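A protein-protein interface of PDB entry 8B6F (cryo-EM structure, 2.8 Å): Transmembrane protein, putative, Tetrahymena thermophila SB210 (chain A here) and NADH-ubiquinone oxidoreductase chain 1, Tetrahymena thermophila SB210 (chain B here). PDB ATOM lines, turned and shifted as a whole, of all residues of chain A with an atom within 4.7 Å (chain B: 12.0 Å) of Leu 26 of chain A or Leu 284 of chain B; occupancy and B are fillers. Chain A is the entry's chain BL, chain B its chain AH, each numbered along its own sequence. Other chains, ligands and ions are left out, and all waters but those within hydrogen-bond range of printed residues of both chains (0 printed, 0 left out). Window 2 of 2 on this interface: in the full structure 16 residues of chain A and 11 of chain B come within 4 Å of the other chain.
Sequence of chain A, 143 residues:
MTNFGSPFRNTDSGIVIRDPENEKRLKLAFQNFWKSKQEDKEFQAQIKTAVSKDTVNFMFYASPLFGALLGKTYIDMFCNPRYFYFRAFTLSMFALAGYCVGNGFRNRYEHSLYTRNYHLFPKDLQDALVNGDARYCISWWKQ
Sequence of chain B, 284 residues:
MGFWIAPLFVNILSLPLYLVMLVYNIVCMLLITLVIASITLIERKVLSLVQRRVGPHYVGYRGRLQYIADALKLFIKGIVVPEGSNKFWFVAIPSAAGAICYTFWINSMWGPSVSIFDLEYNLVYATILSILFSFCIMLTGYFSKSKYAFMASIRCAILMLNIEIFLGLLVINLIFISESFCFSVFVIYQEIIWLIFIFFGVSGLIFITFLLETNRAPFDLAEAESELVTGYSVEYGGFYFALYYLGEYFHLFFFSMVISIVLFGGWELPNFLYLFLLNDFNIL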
ATOM      1  N   ASN A  22      12.109  14.986 -19.430  1.00  0.00           N
ATOM      2  CA  ASN A  22      13.212  15.406 -20.288  1.00  0.00           C
ATOM      3  C   ASN A  22      13.454  16.904 -20.177  1.00  0.00           C
ATOM      4  O   ASN A  22      14.605  17.352 -20.119  1.00  0.00           O
ATOM      5  CB  ASN A  22      12.920  15.019 -21.736  1.00  0.00           C
ATOM      6  CG  ASN A  22      13.961  15.547 -22.700  1.00  0.00           C
ATOM      7  OD1 ASN A  22      15.133  15.682 -22.354  1.00  0.00           O
ATOM      8  ND2 ASN A  22      13.533  15.859 -23.917  1.00  0.00           N
ATOM      9  N   GLU A  23      12.383  17.699 -20.148  1.00  0.00           N
ATOM     10  CA  GLU A  23      12.541  19.142 -20.007  1.00  0.00           C
ATOM     11  C   GLU A  23      13.240  19.489 -18.700  1.00  0.00           C
ATOM     12  O   GLU A  23      14.142  20.333 -18.674  1.00  0.00           O
ATOM     13  CB  GLU A  23      11.179  19.831 -20.084  1.00  0.00           C
ATOM     14  CG  GLU A  23      10.467  19.638 -21.412  1.00  0.00           C
ATOM     15  CD  GLU A  23       9.098  20.292 -21.436  1.00  0.00           C
ATOM     16  OE1 GLU A  23       8.740  20.955 -20.440  1.00  0.00           O
ATOM     17  OE2 GLU A  23       8.382  20.142 -22.448  1.00  0.00           O
ATOM     18  N   LYS A  24      12.835  18.847 -17.602  1.00  0.00           N
ATOM     19  CA  LYS A  24      13.474  19.111 -16.318  1.00  0.00           C
ATOM     20  C   LYS A  24      14.946  18.723 -16.341  1.00  0.00           C
ATOM     21  O   LYS A  24      15.796  19.452 -15.816  1.00  0.00           O
ATOM     22  CB  LYS A  24      12.747  18.357 -15.206  1.00  0.00           C
ATOM     23  CG  LYS A  24      11.374  18.919 -14.875  1.00  0.00           C
ATOM     24  CD  LYS A  24      10.719  18.164 -13.726  1.00  0.00           C
ATOM     25  CE  LYS A  24      11.454  18.387 -12.411  1.00  0.00           C
ATOM     26  NZ  LYS A  24      10.753  17.741 -11.266  1.00  0.00           N
ATOM     27  N   ARG A  25      15.271  17.578 -16.944  1.00  0.00           N
ATOM     28  CA  ARG A  25      16.665  17.156 -17.006  1.00  0.00           C
ATOM     29  C   ARG A  25      17.502  18.147 -17.804  1.00  0.00           C
ATOM     30  O   ARG A  25      18.621  18.488 -17.405  1.00  0.00           O
ATOM     31  CB  ARG A  25      16.765  15.755 -17.610  1.00  0.00           C
ATOM     32  CG  ARG A  25      16.152  14.671 -16.734  1.00  0.00           C
ATOM     33  CD  ARG A  25      16.504  13.272 -17.215  1.00  0.00           C
ATOM     34  NE  ARG A  25      16.254  13.084 -18.640  1.00  0.00           N
ATOM     35  CZ  ARG A  25      16.408  11.933 -19.281  1.00  0.00           C
ATOM     36  NH1 ARG A  25      16.784  10.834 -18.647  1.00  0.00           N
ATOM     37  NH2 ARG A  25      16.182  11.885 -20.590  1.00  0.00           N
ATOM     38  N   LEU A  26      16.976  18.624 -18.933  1.00  0.00           N
ATOM     39  CA  LEU A  26      17.719  19.590 -19.736  1.00  0.00           C
ATOM     40  C   LEU A  26      17.914  20.896 -18.975  1.00  0.00           C
ATOM     41  O   LEU A  26      19.007  21.474 -18.990  1.00  0.00           O
ATOM     42  CB  LEU A  26      16.992  19.840 -21.058  1.00  0.00           C
ATOM     43  CG  LEU A  26      17.885  20.086 -22.279  1.00  0.00           C
ATOM     44  CD1 LEU A  26      17.050  20.256 -23.525  1.00  0.00           C
ATOM     45  CD2 LEU A  26      18.771  21.300 -22.079  1.00  0.00           C
ATOM     46  N   LYS A  27      16.866  21.377 -18.302  1.00  0.00           N
ATOM     47  CA  LYS A  27      16.993  22.601 -17.517  1.00  0.00           C
ATOM     48  C   LYS A  27      18.023  22.436 -16.409  1.00  0.00           C
ATOM     49  O   LYS A  27      18.831  23.338 -16.159  1.00  0.00           O
ATOM     50  CB  LYS A  27      15.637  22.996 -16.931  1.00  0.00           C
ATOM     51  CG  LYS A  27      14.617  23.429 -17.969  1.00  0.00           C
ATOM     52  CD  LYS A  27      13.296  23.811 -17.321  1.00  0.00           C
ATOM     53  CE  LYS A  27      12.232  24.100 -18.368  1.00  0.00           C
ATOM     54  NZ  LYS A  27      12.646  25.176 -19.310  1.00  0.00           N
ATOM     55  N   LEU A  28      18.004  21.290 -15.730  1.00  0.00           N
ATOM     56  CA  LEU A  28      18.983  21.033 -14.680  1.00  0.00           C
ATOM     57  C   LEU A  28      20.397  20.993 -15.243  1.00  0.00           C
ATOM     58  O   LEU A  28      21.332  21.515 -14.627  1.00  0.00           O
ATOM     59  CB  LEU A  28      18.656  19.720 -13.968  1.00  0.00           C
ATOM     60  CG  LEU A  28      19.674  19.251 -12.926  1.00  0.00           C
ATOM     61  CD1 LEU A  28      19.864  20.293 -11.837  1.00  0.00           C
ATOM     62  CD2 LEU A  28      19.239  17.926 -12.325  1.00  0.00           C
ATOM     63  N   ALA A  29      20.573  20.381 -16.414  1.00  0.00           N
ATOM     64  CA  ALA A  29      21.899  20.319 -17.016  1.00  0.00           C
ATOM     65  C   ALA A  29      22.440  21.713 -17.298  1.00  0.00           C
ATOM     66  O   ALA A  29      23.596  22.017 -16.983  1.00  0.00           O
ATOM     67  CB  ALA A  29      21.847  19.496 -18.303  1.00  0.00           C
ATOM     68  N   PHE A  30      21.622  22.580 -17.894  1.00  0.00           N
ATOM     69  CA  PHE A  30      22.096  23.926 -18.195  1.00  0.00           C
ATOM     70  C   PHE A  30      22.299  24.744 -16.928  1.00  0.00           C
ATOM     71  O   PHE A  30      23.225  25.560 -16.862  1.00  0.00           O
ATOM     72  CB  PHE A  30      21.135  24.630 -19.149  1.00  0.00           C
ATOM     73  CG  PHE A  30      21.553  24.540 -20.586  1.00  0.00           C
ATOM     74  CD1 PHE A  30      22.482  25.426 -21.105  1.00  0.00           C
ATOM     75  CD2 PHE A  30      21.042  23.554 -21.410  1.00  0.00           C
ATOM     76  CE1 PHE A  30      22.880  25.339 -22.423  1.00  0.00           C
ATOM     77  CE2 PHE A  30      21.436  23.460 -22.730  1.00  0.00           C
ATOM     78  CZ  PHE A  30      22.356  24.357 -23.237  1.00  0.00           C
ATOM     79  N   TYR A 114      20.672  32.237 -25.118  1.00  0.00           N
ATOM     80  CA  TYR A 114      20.956  30.885 -25.578  1.00  0.00           C
ATOM     81  C   TYR A 114      21.316  30.808 -27.055  1.00  0.00           C
ATOM     82  O   TYR A 114      21.662  29.724 -27.533  1.00  0.00           O
ATOM     83  CB  TYR A 114      19.754  29.982 -25.294  1.00  0.00           C
ATOM     84  CG  TYR A 114      19.680  29.545 -23.853  1.00  0.00           C
ATOM     85  CD1 TYR A 114      20.381  28.433 -23.410  1.00  0.00           C
ATOM     86  CD2 TYR A 114      18.927  30.257 -22.931  1.00  0.00           C
ATOM     87  CE1 TYR A 114      20.325  28.037 -22.090  1.00  0.00           C
ATOM     88  CE2 TYR A 114      18.865  29.869 -21.610  1.00  0.00           C
ATOM     89  CZ  TYR A 114      19.566  28.758 -21.195  1.00  0.00           C
ATOM     90  OH  TYR A 114      19.503  28.370 -19.878  1.00  0.00           O
ATOM     91  N   ALA A 128      22.342  18.990 -27.139  1.00  0.00           N
ATOM     92  CA  ALA A 128      21.166  18.886 -26.282  1.00  0.00           C
ATOM     93  C   ALA A 128      20.261  20.099 -26.442  1.00  0.00           C
ATOM     94  O   ALA A 128      19.033  19.971 -26.435  1.00  0.00           O
ATOM     95  CB  ALA A 128      21.593  18.729 -24.823  1.00  0.00           C
ATOM     96  N   LEU A 129      20.849  21.289 -26.574  1.00  0.00           N
ATOM     97  CA  LEU A 129      20.045  22.491 -26.757  1.00  0.00           C
ATOM     98  C   LEU A 129      19.355  22.493 -28.115  1.00  0.00           C
ATOM     99  O   LEU A 129      18.154  22.773 -28.210  1.00  0.00           O
ATOM    100  CB  LEU A 129      20.924  23.732 -26.600  1.00  0.00           C
ATOM    101  CG  LEU A 129      20.228  25.083 -26.789  1.00  0.00           C
ATOM    102  CD1 LEU A 129      19.102  25.262 -25.786  1.00  0.00           C
ATOM    103  CD2 LEU A 129      21.234  26.213 -26.673  1.00  0.00           C
ATOM    104  N   ASN A 131      18.608  19.993 -30.181  1.00  0.00           N
ATOM    105  CA  ASN A 131      17.581  18.966 -30.220  1.00  0.00           C
ATOM    106  C   ASN A 131      16.745  19.007 -28.946  1.00  0.00           C
ATOM    107  O   ASN A 131      17.119  19.621 -27.946  1.00  0.00           O
ATOM    108  CB  ASN A 131      18.213  17.585 -30.388  1.00  0.00           C
ATOM    109  CG  ASN A 131      19.131  17.509 -31.588  1.00  0.00           C
ATOM    110  OD1 ASN A 131      18.694  17.234 -32.704  1.00  0.00           O
ATOM    111  ND2 ASN A 131      20.418  17.749 -31.363  1.00  0.00           N
ATOM    112  N   GLY A 132      15.597  18.341 -28.995  1.00  0.00           N
ATOM    113  CA  GLY A 132      14.730  18.285 -27.834  1.00  0.00           C
ATOM    114  C   GLY A 132      15.146  17.293 -26.774  1.00  0.00           C
ATOM    115  O   GLY A 132      14.591  17.319 -25.672  1.00  0.00           O
ATOM    116  N   ASP A 133      16.110  16.428 -27.074  1.00  0.00           N
ATOM    117  CA  ASP A 133      16.516  15.374 -26.156  1.00  0.00           C
ATOM    118  C   ASP A 133      17.653  15.844 -25.261  1.00  0.00           C
ATOM    119  O   ASP A 133      18.566  16.542 -25.708  1.00  0.00           O
ATOM    120  CB  ASP A 133      16.952  14.127 -26.926  1.00  0.00           C
ATOM    121  CG  ASP A 133      15.823  13.512 -27.725  1.00  0.00           C
ATOM    122  OD1 ASP A 133      14.674  13.985 -27.597  1.00  0.00           O
ATOM    123  OD2 ASP A 133      16.083  12.554 -28.484  1.00  0.00           O
ATOM    124  N   ALA A 134      17.587  15.453 -23.993  1.00  0.00           N
ATOM    125  CA  ALA A 134      18.667  15.685 -23.047  1.00  0.00           C
ATOM    126  C   ALA A 134      19.654  14.529 -22.999  1.00  0.00           C
ATOM    127  O   ALA A 134      20.611  14.582 -22.219  1.00  0.00           O
ATOM    128  CB  ALA A 134      18.095  15.932 -21.648  1.00  0.00           C
ATOM    129  N   ASN B 279       3.735  32.948 -24.934  1.00  0.00           N
ATOM    130  CA  ASN B 279       5.167  33.166 -25.077  1.00  0.00           C
ATOM    131  C   ASN B 279       5.581  32.862 -26.510  1.00  0.00           C
ATOM    132  O   ASN B 279       5.086  31.910 -27.118  1.00  0.00           O
ATOM    133  CB  ASN B 279       5.957  32.278 -24.115  1.00  0.00           C
ATOM    134  CG  ASN B 279       5.801  32.700 -22.671  1.00  0.00           C
ATOM    135  OD1 ASN B 279       6.539  33.552 -22.179  1.00  0.00           O
ATOM    136  ND2 ASN B 279       4.841  32.099 -21.981  1.00  0.00           N
ATOM    137  N   ASP B 280       6.486  33.676 -27.050  1.00  0.00           N
ATOM    138  CA  ASP B 280       6.895  33.517 -28.440  1.00  0.00           C
ATOM    139  C   ASP B 280       7.994  32.484 -28.638  1.00  0.00           C
ATOM    140  O   ASP B 280       8.240  32.086 -29.781  1.00  0.00           O
ATOM    141  CB  ASP B 280       7.346  34.856 -29.019  1.00  0.00           C
ATOM    142  CG  ASP B 280       6.179  35.762 -29.331  1.00  0.00           C
ATOM    143  OD1 ASP B 280       5.032  35.384 -29.015  1.00  0.00           O
ATOM    144  OD2 ASP B 280       6.396  36.831 -29.926  1.00  0.00           O
ATOM    145  N   PHE B 281       8.653  32.038 -27.574  1.00  0.00           N
ATOM    146  CA  PHE B 281       9.710  31.048 -27.700  1.00  0.00           C
ATOM    147  C   PHE B 281       9.725  30.184 -26.450  1.00  0.00           C
ATOM    148  O   PHE B 281       9.219  30.571 -25.395  1.00  0.00           O
ATOM    149  CB  PHE B 281      11.087  31.697 -27.898  1.00  0.00           C
ATOM    150  CG  PHE B 281      11.208  32.512 -29.153  1.00  0.00           C
ATOM    151  CD1 PHE B 281      11.348  31.897 -30.385  1.00  0.00           C
ATOM    152  CD2 PHE B 281      11.208  33.896 -29.096  1.00  0.00           C
ATOM    153  CE1 PHE B 281      11.467  32.645 -31.539  1.00  0.00           C
ATOM    154  CE2 PHE B 281      11.326  34.650 -30.248  1.00  0.00           C
ATOM    155  CZ  PHE B 281      11.457  34.023 -31.470  1.00  0.00           C
ATOM    156  N   ASN B 282      10.317  29.001 -26.586  1.00  0.00           N
ATOM    157  CA  ASN B 282      10.527  28.097 -25.459  1.00  0.00           C
ATOM    158  C   ASN B 282      11.939  27.542 -25.573  1.00  0.00           C
ATOM    159  O   ASN B 282      12.211  26.694 -26.430  1.00  0.00           O
ATOM    160  CB  ASN B 282       9.489  26.975 -25.441  1.00  0.00           C
ATOM    161  CG  ASN B 282       9.500  26.150 -26.707  1.00  0.00           C
ATOM    162  OD1 ASN B 282       9.948  26.609 -27.755  1.00  0.00           O
ATOM    163  ND2 ASN B 282       9.002  24.923 -26.618  1.00  0.00           N
ATOM    164  N   ILE B 283      12.837  28.033 -24.725  1.00  0.00           N
ATOM    165  CA  ILE B 283      14.229  27.607 -24.704  1.00  0.00           C
ATOM    166  C   ILE B 283      14.504  26.972 -23.350  1.00  0.00           C
ATOM    167  O   ILE B 283      14.235  27.581 -22.308  1.00  0.00           O
ATOM    168  CB  ILE B 283      15.194  28.780 -24.957  1.00  0.00           C
ATOM    169  CG1 ILE B 283      14.834  29.531 -26.242  1.00  0.00           C
ATOM    170  CG2 ILE B 283      16.624  28.284 -25.039  1.00  0.00           C
ATOM    171  CD1 ILE B 283      13.767  30.596 -26.070  1.00  0.00           C
ATOM    172  N   LEU B 284      15.034  25.755 -23.367  1.00  0.00           N
ATOM    173  CA  LEU B 284      15.330  25.032 -22.138  1.00  0.00           C
ATOM    174  C   LEU B 284      16.735  25.354 -21.646  1.00  0.00           C
ATOM    175  O   LEU B 284      17.598  25.761 -22.421  1.00  0.00           O
ATOM    176  CB  LEU B 284      15.175  23.524 -22.358  1.00  0.00           C
ATOM    177  CG  LEU B 284      13.802  23.065 -22.860  1.00  0.00           C
ATOM    178  CD1 LEU B 284      13.770  21.559 -23.091  1.00  0.00           C
ATOM    179  CD2 LEU B 284      12.697  23.476 -21.897  1.00  0.00           C
ATOM    180  OXT LEU B 284      17.041  25.219 -20.462  1.00  0.00           O
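Among the printed residues, merely in contact across the chains: Leu 26 of chain A with Leu 284 of chain B (3.6 Å), Lys 27 of chain A with Leu 284 of chain B (3.1 Å), Tyr 114 of chain A with Ile 283 of chain B (3.5 Å), Tyr 114 of chain A with Leu 284 of chain B (3.6 Å), Leu 129 of chain A with Ile 283 of chain B (3.98 Å) and Leu 129 of chain A with Leu 284 of chain B (3.7 Å).
Leu 26 of chain A touches just one residue of chain B: Leu 284 (3.6 Å). No residue of chain B comes within 4 Å of Asn 22 of chain A. No residue of chain B comes within 4 Å of Glu 23 of chain A. No residue of chain B comes within 4 Å of Arg 25 of chain A. Lys 27 of chain A touches just one residue of chain B: Leu 284. No residue of chain B comes within 4 Å of Leu 28 of chain A. No residue of chain B comes within 4 Å of Ala 29 of chain A. No residue of chain B comes within 4 Å of Phe 30 of chain A. Of chain B, only Ile 283 (3.5 Å) and Leu 284 (3.6 Å) come within 4 Å of Tyr 114 of chain A. No residue of chain B comes within 4 Å of Ala 128 of chain A. No residue of chain B comes within 4 Å of Gly 132 of chain A. Of the printed residues of chain A, Ile 283 of chain B touches Tyr 114 and Leu 129. The nearest residue of chain B that does not touch Leu 26 of chain A is Ile 283 of chain B (7.2 Å). The nearest printed residue of chain A that does not touch Ile 283 of chain B is Lys 27 of chain A (4.2 Å).
Of the 16 printed residues of chain A, 4 touch a printed residue of chain B. Printed residues of chain B that touch a printed residue of chain A: Ile 283 and Leu 284. Hydrophobic or aromatic side chains of chain B that line the printed part of chain A: Ile 283 and Leu 284. Among the printed residues, 6 pairs touch across the chains. Among the printed residues, no Asp or Glu carboxylate lies within 4 Å of a Lys or Arg side-chain nitrogen of the other chain.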
